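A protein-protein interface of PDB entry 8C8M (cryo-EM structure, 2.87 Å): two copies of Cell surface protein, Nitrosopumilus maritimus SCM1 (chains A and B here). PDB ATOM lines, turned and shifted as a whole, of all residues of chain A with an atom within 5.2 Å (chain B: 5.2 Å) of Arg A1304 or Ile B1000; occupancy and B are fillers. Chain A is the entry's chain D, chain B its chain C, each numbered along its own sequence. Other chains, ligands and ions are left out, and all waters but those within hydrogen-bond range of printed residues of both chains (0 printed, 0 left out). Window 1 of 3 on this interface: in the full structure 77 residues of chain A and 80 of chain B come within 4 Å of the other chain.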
ATOM      1  N   ALA A1265      -3.536  13.112 -27.179  1.00  0.00           N
ATOM      2  CA  ALA A1265      -3.836  14.502 -27.582  1.00  0.00           C
ATOM      3  C   ALA A1265      -3.589  15.440 -26.401  1.00  0.00           C
ATOM      4  O   ALA A1265      -4.284  15.300 -25.375  1.00  0.00           O
ATOM      5  CB  ALA A1265      -5.253  14.594 -28.079  1.00  0.00           C
ATOM      6  N   GLU A1266      -2.632  16.352 -26.538  1.00  0.00           N
ATOM      7  CA  GLU A1266      -2.180  17.223 -25.423  1.00  0.00           C
ATOM      8  C   GLU A1266      -3.119  18.430 -25.329  1.00  0.00           C
ATOM      9  O   GLU A1266      -3.588  18.947 -26.347  1.00  0.00           O
ATOM     10  CB  GLU A1266      -0.711  17.646 -25.556  1.00  0.00           C
ATOM     11  CG  GLU A1266       0.288  16.476 -25.562  1.00  0.00           C
ATOM     12  CD  GLU A1266       0.417  15.794 -26.917  1.00  0.00           C
ATOM     13  OE1 GLU A1266      -0.268  16.293 -27.829  1.00  0.00           O
ATOM     14  OE2 GLU A1266       1.151  14.794 -27.059  1.00  0.00           O
ATOM     15  N   THR A1267      -3.379  18.870 -24.116  1.00  0.00           N
ATOM     16  CA  THR A1267      -4.261  20.024 -23.839  1.00  0.00           C
ATOM     17  C   THR A1267      -3.431  21.175 -23.274  1.00  0.00           C
ATOM     18  O   THR A1267      -2.609  20.940 -22.355  1.00  0.00           O
ATOM     19  CB  THR A1267      -5.381  19.614 -22.878  1.00  0.00           C
ATOM     20  OG1 THR A1267      -5.855  18.317 -23.246  1.00  0.00           O
ATOM     21  CG2 THR A1267      -6.507  20.618 -22.885  1.00  0.00           C
ATOM     22  N   PRO A1300     -13.535  23.373 -27.257  1.00  0.00           N
ATOM     23  CA  PRO A1300     -13.591  23.038 -25.833  1.00  0.00           C
ATOM     24  C   PRO A1300     -13.080  24.168 -24.927  1.00  0.00           C
ATOM     25  O   PRO A1300     -12.952  25.273 -25.368  1.00  0.00           O
ATOM     26  CB  PRO A1300     -12.746  21.756 -25.711  1.00  0.00           C
ATOM     27  CG  PRO A1300     -11.895  21.692 -26.955  1.00  0.00           C
ATOM     28  CD  PRO A1300     -12.513  22.608 -27.980  1.00  0.00           C
ATOM     29  N   ASP A1302     -10.275  24.849 -23.881  1.00  0.00           N
ATOM     30  CA  ASP A1302      -8.928  25.336 -24.261  1.00  0.00           C
ATOM     31  C   ASP A1302      -8.402  24.553 -25.465  1.00  0.00           C
ATOM     32  O   ASP A1302      -9.132  23.718 -26.013  1.00  0.00           O
ATOM     33  CB  ASP A1302      -8.001  25.243 -23.051  1.00  0.00           C
ATOM     34  CG  ASP A1302      -7.806  23.822 -22.564  1.00  0.00           C
ATOM     35  OD1 ASP A1302      -8.473  22.919 -23.107  1.00  0.00           O
ATOM     36  OD2 ASP A1302      -6.976  23.626 -21.652  1.00  0.00           O
ATOM     37  N   PHE A1303      -7.158  24.805 -25.851  1.00  0.00           N
ATOM     38  CA  PHE A1303      -6.571  24.216 -27.077  1.00  0.00           C
ATOM     39  C   PHE A1303      -6.509  22.694 -26.967  1.00  0.00           C
ATOM     40  O   PHE A1303      -6.368  22.173 -25.863  1.00  0.00           O
ATOM     41  CB  PHE A1303      -5.184  24.793 -27.339  1.00  0.00           C
ATOM     42  CG  PHE A1303      -5.229  26.116 -28.047  1.00  0.00           C
ATOM     43  CD1 PHE A1303      -5.129  27.298 -27.335  1.00  0.00           C
ATOM     44  CD2 PHE A1303      -5.415  26.177 -29.419  1.00  0.00           C
ATOM     45  CE1 PHE A1303      -5.196  28.518 -27.989  1.00  0.00           C
ATOM     46  CE2 PHE A1303      -5.457  27.397 -30.073  1.00  0.00           C
ATOM     47  CZ  PHE A1303      -5.365  28.565 -29.354  1.00  0.00           C
ATOM     48  N   ARG A1304      -6.606  22.011 -28.098  1.00  0.00           N
ATOM     49  CA  ARG A1304      -6.584  20.533 -28.164  1.00  0.00           C
ATOM     50  C   ARG A1304      -6.049  20.083 -29.516  1.00  0.00           C
ATOM     51  O   ARG A1304      -6.388  20.730 -30.505  1.00  0.00           O
ATOM     52  CB  ARG A1304      -8.000  19.999 -27.973  1.00  0.00           C
ATOM     53  CG  ARG A1304      -8.056  18.478 -27.846  1.00  0.00           C
ATOM     54  CD  ARG A1304      -9.430  17.956 -27.451  1.00  0.00           C
ATOM     55  NE  ARG A1304      -9.841  18.489 -26.157  1.00  0.00           N
ATOM     56  CZ  ARG A1304      -9.310  18.149 -24.991  1.00  0.00           C
ATOM     57  NH1 ARG A1304      -8.358  17.240 -24.936  1.00  0.00           N
ATOM     58  NH2 ARG A1304      -9.729  18.715 -23.879  1.00  0.00           N
ATOM     59  N   GLU A1305      -5.273  19.005 -29.557  1.00  0.00           N
ATOM     60  CA  GLU A1305      -4.691  18.489 -30.818  1.00  0.00           C
ATOM     61  C   GLU A1305      -5.809  17.952 -31.723  1.00  0.00           C
ATOM     62  O   GLU A1305      -6.819  17.446 -31.204  1.00  0.00           O
ATOM     63  CB  GLU A1305      -3.732  17.338 -30.557  1.00  0.00           C
ATOM     64  CG  GLU A1305      -2.248  17.652 -30.575  1.00  0.00           C
ATOM     65  CD  GLU A1305      -1.441  16.378 -30.430  1.00  0.00           C
ATOM     66  OE1 GLU A1305      -0.346  16.211 -31.010  1.00  0.00           O
ATOM     67  OE2 GLU A1305      -1.943  15.512 -29.746  1.00  0.00           O
ATOM     68  N   THR A1306      -5.610  18.026 -33.034  1.00  0.00           N
ATOM     69  CA  THR A1306      -6.546  17.480 -34.044  1.00  0.00           C
ATOM     70  C   THR A1306      -6.064  16.082 -34.427  1.00  0.00           C
ATOM     71  O   THR A1306      -5.937  15.805 -35.636  1.00  0.00           O
ATOM     72  CB  THR A1306      -6.663  18.426 -35.241  1.00  0.00           C
ATOM     73  OG1 THR A1306      -5.500  18.270 -36.055  1.00  0.00           O
ATOM     74  CG2 THR A1306      -6.821  19.875 -34.836  1.00  0.00           C
ATOM     75  N   ILE A1312      -1.022  20.211 -34.262  1.00  0.00           N
ATOM     76  CA  ILE A1312      -1.979  21.273 -34.673  1.00  0.00           C
ATOM     77  C   ILE A1312      -3.087  21.320 -33.625  1.00  0.00           C
ATOM     78  O   ILE A1312      -3.700  20.290 -33.367  1.00  0.00           O
ATOM     79  CB  ILE A1312      -2.514  21.017 -36.089  1.00  0.00           C
ATOM     80  CG1 ILE A1312      -1.377  21.022 -37.112  1.00  0.00           C
ATOM     81  CG2 ILE A1312      -3.604  22.023 -36.432  1.00  0.00           C
ATOM     82  CD1 ILE A1312      -1.775  20.481 -38.473  1.00  0.00           C
ATOM     83  N   PHE A1313      -3.340  22.493 -33.064  1.00  0.00           N
ATOM     84  CA  PHE A1313      -4.351  22.699 -32.001  1.00  0.00           C
ATOM     85  C   PHE A1313      -5.443  23.635 -32.507  1.00  0.00           C
ATOM     86  O   PHE A1313      -5.132  24.638 -33.166  1.00  0.00           O
ATOM     87  CB  PHE A1313      -3.702  23.257 -30.738  1.00  0.00           C
ATOM     88  CG  PHE A1313      -2.616  22.382 -30.178  1.00  0.00           C
ATOM     89  CD1 PHE A1313      -1.342  22.398 -30.732  1.00  0.00           C
ATOM     90  CD2 PHE A1313      -2.853  21.551 -29.091  1.00  0.00           C
ATOM     91  CE1 PHE A1313      -0.338  21.583 -30.232  1.00  0.00           C
ATOM     92  CE2 PHE A1313      -1.842  20.748 -28.582  1.00  0.00           C
ATOM     93  CZ  PHE A1313      -0.587  20.764 -29.155  1.00  0.00           C
ATOM     94  N   GLN A1314      -6.688  23.332 -32.164  1.00  0.00           N
ATOM     95  CA  GLN A1314      -7.856  24.108 -32.623  1.00  0.00           C
ATOM     96  C   GLN A1314      -8.750  24.441 -31.434  1.00  0.00           C
ATOM     97  O   GLN A1314      -8.858  23.628 -30.515  1.00  0.00           O
ATOM     98  CB  GLN A1314      -8.610  23.338 -33.698  1.00  0.00           C
ATOM     99  CG  GLN A1314      -7.907  23.399 -35.041  1.00  0.00           C
ATOM    100  CD  GLN A1314      -8.760  22.939 -36.197  1.00  0.00           C
ATOM    101  OE1 GLN A1314      -9.763  22.248 -36.024  1.00  0.00           O
ATOM    102  NE2 GLN A1314      -8.339  23.303 -37.399  1.00  0.00           N
ATOM    103  N   VAL B 732      -6.454  15.413 -16.564  1.00  0.00           N
ATOM    104  CA  VAL B 732      -6.549  15.716 -18.019  1.00  0.00           C
ATOM    105  C   VAL B 732      -5.475  14.927 -18.772  1.00  0.00           C
ATOM    106  O   VAL B 732      -5.804  14.346 -19.817  1.00  0.00           O
ATOM    107  CB  VAL B 732      -6.451  17.227 -18.284  1.00  0.00           C
ATOM    108  CG1 VAL B 732      -6.319  17.545 -19.767  1.00  0.00           C
ATOM    109  CG2 VAL B 732      -7.651  17.952 -17.690  1.00  0.00           C
ATOM    110  N   ARG B 737      -3.997   9.519 -14.914  1.00  0.00           N
ATOM    111  CA  ARG B 737      -5.141   8.611 -14.645  1.00  0.00           C
ATOM    112  C   ARG B 737      -4.632   7.204 -14.355  1.00  0.00           C
ATOM    113  O   ARG B 737      -3.760   6.743 -15.114  1.00  0.00           O
ATOM    114  CB  ARG B 737      -6.039   8.585 -15.872  1.00  0.00           C
ATOM    115  CG  ARG B 737      -6.421   9.972 -16.357  1.00  0.00           C
ATOM    116  CD  ARG B 737      -7.643   9.953 -17.243  1.00  0.00           C
ATOM    117  NE  ARG B 737      -7.273  10.037 -18.644  1.00  0.00           N
ATOM    118  CZ  ARG B 737      -7.499  11.065 -19.463  1.00  0.00           C
ATOM    119  NH1 ARG B 737      -8.094  12.172 -19.046  1.00  0.00           N
ATOM    120  NH2 ARG B 737      -7.111  10.973 -20.723  1.00  0.00           N
ATOM    121  N   PHE B 886     -10.845  22.080 -16.763  1.00  0.00           N
ATOM    122  CA  PHE B 886     -11.797  21.954 -17.897  1.00  0.00           C
ATOM    123  C   PHE B 886     -13.128  22.590 -17.501  1.00  0.00           C
ATOM    124  O   PHE B 886     -13.881  23.028 -18.359  1.00  0.00           O
ATOM    125  CB  PHE B 886     -11.965  20.497 -18.326  1.00  0.00           C
ATOM    126  CG  PHE B 886     -12.433  19.596 -17.220  1.00  0.00           C
ATOM    127  CD1 PHE B 886     -11.519  18.949 -16.404  1.00  0.00           C
ATOM    128  CD2 PHE B 886     -13.784  19.445 -16.967  1.00  0.00           C
ATOM    129  CE1 PHE B 886     -11.952  18.136 -15.370  1.00  0.00           C
ATOM    130  CE2 PHE B 886     -14.219  18.633 -15.934  1.00  0.00           C
ATOM    131  CZ  PHE B 886     -13.301  17.978 -15.144  1.00  0.00           C
ATOM    132  N   VAL B 991     -21.535  17.476 -21.707  1.00  0.00           N
ATOM    133  CA  VAL B 991     -20.062  17.395 -21.512  1.00  0.00           C
ATOM    134  C   VAL B 991     -19.668  15.928 -21.523  1.00  0.00           C
ATOM    135  O   VAL B 991     -20.050  15.198 -20.607  1.00  0.00           O
ATOM    136  CB  VAL B 991     -19.602  18.064 -20.218  1.00  0.00           C
ATOM    137  CG1 VAL B 991     -18.102  17.870 -20.009  1.00  0.00           C
ATOM    138  CG2 VAL B 991     -19.976  19.539 -20.214  1.00  0.00           C
ATOM    139  N   ASP B 992     -18.910  15.540 -22.542  1.00  0.00           N
ATOM    140  CA  ASP B 992     -18.391  14.164 -22.674  1.00  0.00           C
ATOM    141  C   ASP B 992     -17.090  14.071 -21.888  1.00  0.00           C
ATOM    142  O   ASP B 992     -16.108  14.687 -22.306  1.00  0.00           O
ATOM    143  CB  ASP B 992     -18.202  13.756 -24.136  1.00  0.00           C
ATOM    144  CG  ASP B 992     -18.158  12.254 -24.250  1.00  0.00           C
ATOM    145  OD1 ASP B 992     -18.393  11.597 -23.197  1.00  0.00           O
ATOM    146  OD2 ASP B 992     -17.867  11.767 -25.354  1.00  0.00           O
ATOM    147  N   PHE B 993     -17.087  13.312 -20.798  1.00  0.00           N
ATOM    148  CA  PHE B 993     -15.860  13.054 -20.019  1.00  0.00           C
ATOM    149  C   PHE B 993     -14.871  12.266 -20.891  1.00  0.00           C
ATOM    150  O   PHE B 993     -13.660  12.394 -20.676  1.00  0.00           O
ATOM    151  CB  PHE B 993     -16.192  12.322 -18.726  1.00  0.00           C
ATOM    152  CG  PHE B 993     -15.131  12.464 -17.676  1.00  0.00           C
ATOM    153  CD1 PHE B 993     -14.602  13.716 -17.388  1.00  0.00           C
ATOM    154  CD2 PHE B 993     -14.665  11.364 -16.975  1.00  0.00           C
ATOM    155  CE1 PHE B 993     -13.612  13.872 -16.431  1.00  0.00           C
ATOM    156  CE2 PHE B 993     -13.687  11.521 -16.008  1.00  0.00           C
ATOM    157  CZ  PHE B 993     -13.169  12.770 -15.731  1.00  0.00           C
ATOM    158  N   ARG B 994     -15.358  11.478 -21.852  1.00  0.00           N
ATOM    159  CA  ARG B 994     -14.486  10.650 -22.716  1.00  0.00           C
ATOM    160  C   ARG B 994     -14.987  10.712 -24.148  1.00  0.00           C
ATOM    161  O   ARG B 994     -15.997  10.042 -24.420  1.00  0.00           O
ATOM    162  CB  ARG B 994     -14.496   9.213 -22.211  1.00  0.00           C
ATOM    163  CG  ARG B 994     -13.905   9.042 -20.818  1.00  0.00           C
ATOM    164  CD  ARG B 994     -12.422   9.373 -20.857  1.00  0.00           C
ATOM    165  NE  ARG B 994     -11.787   9.104 -19.576  1.00  0.00           N
ATOM    166  CZ  ARG B 994     -11.389  10.011 -18.683  1.00  0.00           C
ATOM    167  NH1 ARG B 994     -11.538  11.313 -18.899  1.00  0.00           N
ATOM    168  NH2 ARG B 994     -10.853   9.594 -17.548  1.00  0.00           N
ATOM    169  N   ASP B 995     -14.287  11.457 -25.004  1.00  0.00           N
ATOM    170  CA  ASP B 995     -14.597  11.541 -26.455  1.00  0.00           C
ATOM    171  C   ASP B 995     -13.900  10.363 -27.153  1.00  0.00           C
ATOM    172  O   ASP B 995     -13.408   9.464 -26.464  1.00  0.00           O
ATOM    173  CB  ASP B 995     -14.177  12.909 -26.991  1.00  0.00           C
ATOM    174  CG  ASP B 995     -12.657  13.068 -27.046  1.00  0.00           C
ATOM    175  OD1 ASP B 995     -12.122  13.299 -28.150  1.00  0.00           O
ATOM    176  OD2 ASP B 995     -12.026  12.912 -25.999  1.00  0.00           O
ATOM    177  N   GLY B 998     -10.544   9.991 -25.560  1.00  0.00           N
ATOM    178  CA  GLY B 998     -10.538   9.836 -24.100  1.00  0.00           C
ATOM    179  C   GLY B 998     -10.180  11.153 -23.461  1.00  0.00           C
ATOM    180  O   GLY B 998      -9.607  11.126 -22.386  1.00  0.00           O
ATOM    181  N   GLU B 999     -10.686  12.247 -24.011  1.00  0.00           N
ATOM    182  CA  GLU B 999     -10.423  13.613 -23.541  1.00  0.00           C
ATOM    183  C   GLU B 999     -11.759  14.330 -23.288  1.00  0.00           C
ATOM    184  O   GLU B 999     -12.760  13.841 -23.759  1.00  0.00           O
ATOM    185  CB  GLU B 999      -9.507  14.236 -24.590  1.00  0.00           C
ATOM    186  CG  GLU B 999      -8.067  14.313 -24.098  1.00  0.00           C
ATOM    187  CD  GLU B 999      -7.158  13.119 -24.194  1.00  0.00           C
ATOM    188  OE1 GLU B 999      -6.924  12.707 -25.315  1.00  0.00           O
ATOM    189  OE2 GLU B 999      -6.651  12.669 -23.148  1.00  0.00           O
ATOM    190  N   ILE B1000     -11.771  15.430 -22.540  1.00  0.00           N
ATOM    191  CA  ILE B1000     -13.051  16.100 -22.180  1.00  0.00           C
ATOM    192  C   ILE B1000     -13.388  17.114 -23.277  1.00  0.00           C
ATOM    193  O   ILE B1000     -12.482  17.815 -23.715  1.00  0.00           O
ATOM    194  CB  ILE B1000     -12.990  16.714 -20.777  1.00  0.00           C
ATOM    195  CG1 ILE B1000     -12.556  15.677 -19.745  1.00  0.00           C
ATOM    196  CG2 ILE B1000     -14.342  17.289 -20.387  1.00  0.00           C
ATOM    197  CD1 ILE B1000     -11.206  15.881 -19.154  1.00  0.00           C
ATOM    198  N   VAL B1001     -14.624  17.104 -23.758  1.00  0.00           N
ATOM    199  CA  VAL B1001     -15.116  18.060 -24.784  1.00  0.00           C
ATOM    200  C   VAL B1001     -16.560  18.377 -24.444  1.00  0.00           C
ATOM    201  O   VAL B1001     -17.191  17.555 -23.839  1.00  0.00           O
ATOM    202  CB  VAL B1001     -14.985  17.490 -26.202  1.00  0.00           C
ATOM    203  CG1 VAL B1001     -16.037  16.442 -26.502  1.00  0.00           C
ATOM    204  CG2 VAL B1001     -15.029  18.594 -27.244  1.00  0.00           C
ATOM    205  N   GLU B1002     -17.074  19.524 -24.847  1.00  0.00           N
ATOM    206  CA  GLU B1002     -18.504  19.854 -24.641  1.00  0.00           C
ATOM    207  C   GLU B1002     -19.163  20.016 -26.009  1.00  0.00           C
ATOM    208  O   GLU B1002     -18.583  20.666 -26.884  1.00  0.00           O
ATOM    209  CB  GLU B1002     -18.607  21.101 -23.776  1.00  0.00           C
ATOM    210  CG  GLU B1002     -20.018  21.626 -23.608  1.00  0.00           C
ATOM    211  CD  GLU B1002     -20.058  23.062 -23.107  1.00  0.00           C
ATOM    212  OE1 GLU B1002     -19.244  23.881 -23.585  1.00  0.00           O
ATOM    213  OE2 GLU B1002     -20.896  23.359 -22.245  1.00  0.00           O
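Of chain B, only Glu B999 and Ile B1000 come within 4 Å of Arg A1304. Of chain A, only Arg A1304 (2.9 Å) comes within 4 Å of Ile B1000. Of the printed residues of chain B, Thr A1267 touches Val B732 (3.6 Å). Printed residues of chain A within 4 Å of Val B732: Thr A1267 (3.6 Å). Thr A1306 touches none of the printed residues of chain B. The nearest printed residue of chain B that does not touch Arg A1304 is Val B1001 (5.2 Å). The nearest residue of chain A that does not touch Ile B1000 is Pro A1300 (4.4 Å).
No position is printed for both chains. Of the 4 pairs that touch across the chains among the printed residues, none has its exchanged pair printed and touching as well.
Glu B999 touches Ala A1265. CG1 of Val B732 touches OG1 of Thr A1267, at 3.6 Å. Glu B999 touches Arg A1304.
The guanidinium group of Arg B737 is in salt-bridge range of the side-chain carboxylate of Glu B999 (3.0 Å). The backbone NH (N) of Gln A1314 sits at hydrogen-bond distance from the backbone carbonyl oxygen (O) of Arg A1304 (3.1 Å). The side-chain hydroxyl (OG1) of Thr A1267 lies within hydrogen-bond range of the guanidinium group (NH1) of Arg A1304. The backbone NH (N) of Glu B999 sits at hydrogen-bond distance from the side-chain carboxylate (OD2) of Asp B995, at 2.5 Å. The guanidinium group of Arg B737 lies within hydrogen-bond range of the backbone carbonyl oxygen of Val B732, at 3.3 Å.
Hydrophobic or aromatic side chains of chain A that line the printed part of chain B: Ala A1265. Of the 13 printed residues of chain B, 3 touch a printed residue of chain A. Hydrophobic or aromatic side chains of chain B that line the printed part of chain A: Val B732. Among the printed residues, no Asp or Glu carboxylate lies within 4 Å of a Lys or Arg side-chain nitrogen of the other chain.
The backbone carbonyl oxygen (O) of Ile B1000 lies within hydrogen-bond range of the guanidinium group (NH2) of Arg A1304 (2.9 Å).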
